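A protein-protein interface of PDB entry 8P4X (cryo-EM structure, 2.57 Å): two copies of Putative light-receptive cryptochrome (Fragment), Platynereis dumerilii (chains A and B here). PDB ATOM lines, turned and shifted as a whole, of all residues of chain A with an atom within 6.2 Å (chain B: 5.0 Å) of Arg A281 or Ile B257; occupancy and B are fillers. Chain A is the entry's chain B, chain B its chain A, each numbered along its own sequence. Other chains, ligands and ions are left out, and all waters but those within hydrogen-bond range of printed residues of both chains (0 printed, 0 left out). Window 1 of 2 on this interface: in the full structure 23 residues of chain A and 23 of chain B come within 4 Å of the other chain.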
ATOM      1  N   TRP A 240      18.747 -13.309  13.977  1.00  0.00           N
ATOM      2  CA  TRP A 240      18.548 -11.889  14.219  1.00  0.00           C
ATOM      3  C   TRP A 240      19.839 -11.130  13.946  1.00  0.00           C
ATOM      4  O   TRP A 240      20.940 -11.653  14.141  1.00  0.00           O
ATOM      5  CB  TRP A 240      18.095 -11.631  15.661  1.00  0.00           C
ATOM      6  CG  TRP A 240      16.732 -12.159  15.976  1.00  0.00           C
ATOM      7  CD1 TRP A 240      16.403 -13.445  16.283  1.00  0.00           C
ATOM      8  CD2 TRP A 240      15.513 -11.412  16.025  1.00  0.00           C
ATOM      9  NE1 TRP A 240      15.055 -13.547  16.514  1.00  0.00           N
ATOM     10  CE2 TRP A 240      14.485 -12.312  16.363  1.00  0.00           C
ATOM     11  CE3 TRP A 240      15.189 -10.069  15.814  1.00  0.00           C
ATOM     12  CZ2 TRP A 240      13.159 -11.912  16.494  1.00  0.00           C
ATOM     13  CZ3 TRP A 240      13.875  -9.677  15.944  1.00  0.00           C
ATOM     14  CH2 TRP A 240      12.876 -10.593  16.281  1.00  0.00           C
ATOM     15  N   LEU A 250      13.532  -3.049   7.393  1.00  0.00           N
ATOM     16  CA  LEU A 250      12.304  -3.590   7.963  1.00  0.00           C
ATOM     17  C   LEU A 250      11.178  -2.565   7.915  1.00  0.00           C
ATOM     18  O   LEU A 250      10.025  -2.911   7.633  1.00  0.00           O
ATOM     19  CB  LEU A 250      12.556  -4.044   9.400  1.00  0.00           C
ATOM     20  CG  LEU A 250      13.325  -5.351   9.585  1.00  0.00           C
ATOM     21  CD1 LEU A 250      13.784  -5.495  11.022  1.00  0.00           C
ATOM     22  CD2 LEU A 250      12.470  -6.539   9.189  1.00  0.00           C
ATOM     23  N   THR A 253       9.851  -2.389   4.333  1.00  0.00           N
ATOM     24  CA  THR A 253       9.020  -3.552   4.040  1.00  0.00           C
ATOM     25  C   THR A 253       7.654  -3.442   4.706  1.00  0.00           C
ATOM     26  O   THR A 253       6.626  -3.715   4.071  1.00  0.00           O
ATOM     27  CB  THR A 253       9.734  -4.829   4.489  1.00  0.00           C
ATOM     28  OG1 THR A 253      11.036  -4.884   3.900  1.00  0.00           O
ATOM     29  CG2 THR A 253       8.953  -6.056   4.073  1.00  0.00           C
ATOM     30  N   ARG A 254       7.629  -3.032   5.977  1.00  0.00           N
ATOM     31  CA  ARG A 254       6.366  -2.826   6.677  1.00  0.00           C
ATOM     32  C   ARG A 254       5.489  -1.821   5.944  1.00  0.00           C
ATOM     33  O   ARG A 254       4.288  -2.052   5.761  1.00  0.00           O
ATOM     34  CB  ARG A 254       6.646  -2.357   8.108  1.00  0.00           C
ATOM     35  CG  ARG A 254       5.423  -1.983   8.927  1.00  0.00           C
ATOM     36  CD  ARG A 254       4.596  -3.193   9.308  1.00  0.00           C
ATOM     37  NE  ARG A 254       5.098  -3.836  10.516  1.00  0.00           N
ATOM     38  CZ  ARG A 254       4.838  -3.418  11.747  1.00  0.00           C
ATOM     39  NH1 ARG A 254       4.097  -2.346  11.972  1.00  0.00           N
ATOM     40  NH2 ARG A 254       5.335  -4.092  12.780  1.00  0.00           N
ATOM     41  N   ILE A 257       4.088  -3.277   2.600  1.00  0.00           N
ATOM     42  CA  ILE A 257       3.059  -4.269   2.880  1.00  0.00           C
ATOM     43  C   ILE A 257       1.734  -3.591   3.208  1.00  0.00           C
ATOM     44  O   ILE A 257       0.678  -3.978   2.689  1.00  0.00           O
ATOM     45  CB  ILE A 257       3.517  -5.190   4.024  1.00  0.00           C
ATOM     46  CG1 ILE A 257       4.616  -6.132   3.537  1.00  0.00           C
ATOM     47  CG2 ILE A 257       2.336  -5.970   4.576  1.00  0.00           C
ATOM     48  CD1 ILE A 257       5.297  -6.914   4.639  1.00  0.00           C
ATOM     49  N   PRO A 279       8.779 -15.795   9.387  1.00  0.00           N
ATOM     50  CA  PRO A 279       9.672 -14.766   9.934  1.00  0.00           C
ATOM     51  C   PRO A 279       8.913 -13.795  10.822  1.00  0.00           C
ATOM     52  O   PRO A 279       7.774 -13.419  10.509  1.00  0.00           O
ATOM     53  CB  PRO A 279      10.215 -14.069   8.678  1.00  0.00           C
ATOM     54  CG  PRO A 279      10.075 -15.072   7.599  1.00  0.00           C
ATOM     55  CD  PRO A 279       8.845 -15.859   7.918  1.00  0.00           C
ATOM     56  N   PRO A 280       9.509 -13.360  11.944  1.00  0.00           N
ATOM     57  CA  PRO A 280       8.812 -12.408  12.824  1.00  0.00           C
ATOM     58  C   PRO A 280       8.578 -11.046  12.190  1.00  0.00           C
ATOM     59  O   PRO A 280       7.449 -10.544  12.194  1.00  0.00           O
ATOM     60  CB  PRO A 280       9.747 -12.301  14.035  1.00  0.00           C
ATOM     61  CG  PRO A 280      10.562 -13.533  14.005  1.00  0.00           C
ATOM     62  CD  PRO A 280      10.750 -13.858  12.563  1.00  0.00           C
ATOM     63  N   ARG A 281       9.634 -10.434  11.654  1.00  0.00           N
ATOM     64  CA  ARG A 281       9.559  -9.089  11.084  1.00  0.00           C
ATOM     65  C   ARG A 281       9.174  -8.068  12.153  1.00  0.00           C
ATOM     66  O   ARG A 281       8.190  -7.337  12.024  1.00  0.00           O
ATOM     67  CB  ARG A 281       8.579  -9.044   9.909  1.00  0.00           C
ATOM     68  CG  ARG A 281       8.829 -10.085   8.837  1.00  0.00           C
ATOM     69  CD  ARG A 281       7.765 -10.018   7.754  1.00  0.00           C
ATOM     70  NE  ARG A 281       7.751 -11.207   6.907  1.00  0.00           N
ATOM     71  CZ  ARG A 281       8.512 -11.376   5.834  1.00  0.00           C
ATOM     72  NH1 ARG A 281       9.376 -10.456   5.446  1.00  0.00           N
ATOM     73  NH2 ARG A 281       8.403 -12.500   5.134  1.00  0.00           N
ATOM     74  N   SER A 282       9.968  -8.018  13.220  1.00  0.00           N
ATOM     75  CA  SER A 282       9.700  -7.171  14.374  1.00  0.00           C
ATOM     76  C   SER A 282      10.847  -6.193  14.581  1.00  0.00           C
ATOM     77  O   SER A 282      12.001  -6.499  14.262  1.00  0.00           O
ATOM     78  CB  SER A 282       9.496  -8.014  15.638  1.00  0.00           C
ATOM     79  OG  SER A 282       9.315  -7.198  16.778  1.00  0.00           O
ATOM     80  N   MET A 283      10.523  -5.016  15.116  1.00  0.00           N
ATOM     81  CA  MET A 283      11.500  -3.964  15.372  1.00  0.00           C
ATOM     82  C   MET A 283      11.546  -3.538  16.836  1.00  0.00           C
ATOM     83  O   MET A 283      12.146  -2.505  17.147  1.00  0.00           O
ATOM     84  CB  MET A 283      11.204  -2.750  14.489  1.00  0.00           C
ATOM     85  CG  MET A 283      11.655  -2.898  13.044  1.00  0.00           C
ATOM     86  SD  MET A 283      11.145  -1.524  11.997  1.00  0.00           S
ATOM     87  CE  MET A 283       9.386  -1.826  11.877  1.00  0.00           C
ATOM     88  N   GLU B 252       8.000  -5.153  -6.611  1.00  0.00           N
ATOM     89  CA  GLU B 252       8.899  -4.623  -5.588  1.00  0.00           C
ATOM     90  C   GLU B 252       8.579  -5.211  -4.216  1.00  0.00           C
ATOM     91  O   GLU B 252       9.486  -5.609  -3.464  1.00  0.00           O
ATOM     92  CB  GLU B 252       8.799  -3.099  -5.553  1.00  0.00           C
ATOM     93  CG  GLU B 252       9.415  -2.401  -6.753  1.00  0.00           C
ATOM     94  CD  GLU B 252       9.088  -0.920  -6.801  1.00  0.00           C
ATOM     95  OE1 GLU B 252       9.000  -0.366  -7.917  1.00  0.00           O
ATOM     96  OE2 GLU B 252       8.914  -0.311  -5.724  1.00  0.00           O
ATOM     97  N   THR B 253       7.291  -5.260  -3.868  1.00  0.00           N
ATOM     98  CA  THR B 253       6.891  -5.826  -2.584  1.00  0.00           C
ATOM     99  C   THR B 253       7.293  -7.292  -2.475  1.00  0.00           C
ATOM    100  O   THR B 253       7.824  -7.718  -1.439  1.00  0.00           O
ATOM    101  CB  THR B 253       5.381  -5.669  -2.392  1.00  0.00           C
ATOM    102  OG1 THR B 253       5.015  -4.296  -2.557  1.00  0.00           O
ATOM    103  CG2 THR B 253       4.965  -6.126  -1.011  1.00  0.00           C
ATOM    104  N   ARG B 254       7.058  -8.068  -3.536  1.00  0.00           N
ATOM    105  CA  ARG B 254       7.472  -9.466  -3.554  1.00  0.00           C
ATOM    106  C   ARG B 254       8.972  -9.598  -3.322  1.00  0.00           C
ATOM    107  O   ARG B 254       9.413 -10.435  -2.527  1.00  0.00           O
ATOM    108  CB  ARG B 254       7.075 -10.100  -4.891  1.00  0.00           C
ATOM    109  CG  ARG B 254       7.549 -11.527  -5.107  1.00  0.00           C
ATOM    110  CD  ARG B 254       6.813 -12.515  -4.229  1.00  0.00           C
ATOM    111  NE  ARG B 254       5.553 -12.939  -4.826  1.00  0.00           N
ATOM    112  CZ  ARG B 254       5.446 -13.872  -5.762  1.00  0.00           C
ATOM    113  NH1 ARG B 254       6.510 -14.490  -6.247  1.00  0.00           N
ATOM    114  NH2 ARG B 254       4.242 -14.192  -6.224  1.00  0.00           N
ATOM    115  N   LEU B 255       9.773  -8.776  -4.004  1.00  0.00           N
ATOM    116  CA  LEU B 255      11.223  -8.911  -3.898  1.00  0.00           C
ATOM    117  C   LEU B 255      11.708  -8.607  -2.487  1.00  0.00           C
ATOM    118  O   LEU B 255      12.541  -9.339  -1.939  1.00  0.00           O
ATOM    119  CB  LEU B 255      11.914  -7.997  -4.908  1.00  0.00           C
ATOM    120  CG  LEU B 255      11.749  -8.348  -6.387  1.00  0.00           C
ATOM    121  CD1 LEU B 255      12.517  -7.362  -7.244  1.00  0.00           C
ATOM    122  CD2 LEU B 255      12.193  -9.766  -6.700  1.00  0.00           C
ATOM    123  N   MET B 256      11.201  -7.534  -1.879  1.00  0.00           N
ATOM    124  CA  MET B 256      11.665  -7.198  -0.538  1.00  0.00           C
ATOM    125  C   MET B 256      11.169  -8.187   0.514  1.00  0.00           C
ATOM    126  O   MET B 256      11.895  -8.464   1.481  1.00  0.00           O
ATOM    127  CB  MET B 256      11.240  -5.780  -0.176  1.00  0.00           C
ATOM    128  CG  MET B 256      11.799  -4.718  -1.115  1.00  0.00           C
ATOM    129  SD  MET B 256      12.199  -3.188  -0.261  1.00  0.00           S
ATOM    130  CE  MET B 256      10.689  -2.982   0.671  1.00  0.00           C
ATOM    131  N   ILE B 257       9.957  -8.727   0.358  1.00  0.00           N
ATOM    132  CA  ILE B 257       9.524  -9.791   1.254  1.00  0.00           C
ATOM    133  C   ILE B 257      10.499 -10.961   1.208  1.00  0.00           C
ATOM    134  O   ILE B 257      10.903 -11.491   2.253  1.00  0.00           O
ATOM    135  CB  ILE B 257       8.097 -10.234   0.891  1.00  0.00           C
ATOM    136  CG1 ILE B 257       7.089  -9.162   1.306  1.00  0.00           C
ATOM    137  CG2 ILE B 257       7.775 -11.566   1.550  1.00  0.00           C
ATOM    138  CD1 ILE B 257       5.688  -9.394   0.784  1.00  0.00           C
ATOM    139  N   GLU B 258      10.892 -11.383   0.006  1.00  0.00           N
ATOM    140  CA  GLU B 258      11.833 -12.486  -0.134  1.00  0.00           C
ATOM    141  C   GLU B 258      13.194 -12.141   0.457  1.00  0.00           C
ATOM    142  O   GLU B 258      13.844 -13.001   1.057  1.00  0.00           O
ATOM    143  CB  GLU B 258      11.978 -12.870  -1.606  1.00  0.00           C
ATOM    144  CG  GLU B 258      10.710 -13.393  -2.252  1.00  0.00           C
ATOM    145  CD  GLU B 258      10.346 -14.789  -1.787  1.00  0.00           C
ATOM    146  OE1 GLU B 258      10.946 -15.266  -0.802  1.00  0.00           O
ATOM    147  OE2 GLU B 258       9.462 -15.412  -2.412  1.00  0.00           O
ATOM    148  N   ARG B 259      13.649 -10.901   0.280  1.00  0.00           N
ATOM    149  CA  ARG B 259      14.924 -10.493   0.864  1.00  0.00           C
ATOM    150  C   ARG B 259      14.893 -10.621   2.384  1.00  0.00           C
ATOM    151  O   ARG B 259      15.819 -11.171   2.999  1.00  0.00           O
ATOM    152  CB  ARG B 259      15.247  -9.059   0.446  1.00  0.00           C
ATOM    153  CG  ARG B 259      16.446  -8.448   1.141  1.00  0.00           C
ATOM    154  CD  ARG B 259      16.672  -7.025   0.674  1.00  0.00           C
ATOM    155  NE  ARG B 259      17.211  -6.972  -0.680  1.00  0.00           N
ATOM    156  CZ  ARG B 259      18.486  -6.757  -0.982  1.00  0.00           C
ATOM    157  NH1 ARG B 259      19.397  -6.548  -0.046  1.00  0.00           N
ATOM    158  NH2 ARG B 259      18.856  -6.746  -2.259  1.00  0.00           N
ATOM    159  N   THR B 260      13.828 -10.114   3.007  1.00  0.00           N
ATOM    160  CA  THR B 260      13.707 -10.228   4.455  1.00  0.00           C
ATOM    161  C   THR B 260      13.639 -11.686   4.898  1.00  0.00           C
ATOM    162  O   THR B 260      14.281 -12.061   5.889  1.00  0.00           O
ATOM    163  CB  THR B 260      12.478  -9.453   4.933  1.00  0.00           C
ATOM    164  OG1 THR B 260      12.668  -8.057   4.675  1.00  0.00           O
ATOM    165  CG2 THR B 260      12.254  -9.658   6.416  1.00  0.00           C
ATOM    166  N   ALA B 261      12.890 -12.522   4.177  1.00  0.00           N
ATOM    167  CA  ALA B 261      12.832 -13.941   4.514  1.00  0.00           C
ATOM    168  C   ALA B 261      14.201 -14.607   4.402  1.00  0.00           C
ATOM    169  O   ALA B 261      14.570 -15.416   5.260  1.00  0.00           O
ATOM    170  CB  ALA B 261      11.819 -14.654   3.620  1.00  0.00           C
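O of Met B256 lies within hydrogen-bond range of OG1 of Thr B260 (3.3 Å).
Among the printed residues, pairs that only touch across the chains: Thr A253 with Met B256 (3.8 Å), Thr A253 with Thr B260 (3.7 Å), Arg A281 with Ile B257 (3.7 Å) and Arg A281 with Thr B260 (3.1 Å).
Of chain B, only Ile B257 (3.7 Å) and Thr B260 (3.1 Å) come within 4 Å of Arg A281. Ile B257 touches one residue of chain A. Of the printed residues of chain A, Thr B260 touches Thr A253 and Arg A281. Of the printed residues of chain A, Met B256 touches Thr A253 (3.8 Å). Arg B259 touches none of the printed residues of chain A. Leu A250 touches none of the printed residues of chain B. The nearest residue of chain B that does not touch Arg A281 is Ala B261 (4.3 Å). The nearest residue of chain A that does not touch Ile B257 is Ile A257 (4.4 Å).
Along chain A the printed residues that touch a printed residue of chain B span positions 253 to 281. Of the 10 printed residues of chain B, 3 touch a printed residue of chain A. Printed residues of chain B that touch a printed residue of chain A: Met B256, Ile B257 and Thr B260. Hydrophobic or aromatic side chains of chain B within 4 Å of the printed part of chain A: Met B256 and Ile B257. Among the printed residues, no Asp or Glu carboxylate lies within 4 Å of a Lys or Arg side-chain nitrogen of the other chain.
Positions printed for both chains: 253, 254 and 257. Of the 4 pairs that touch across the chains among the printed residues, none has its exchanged pair printed and touching as well.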
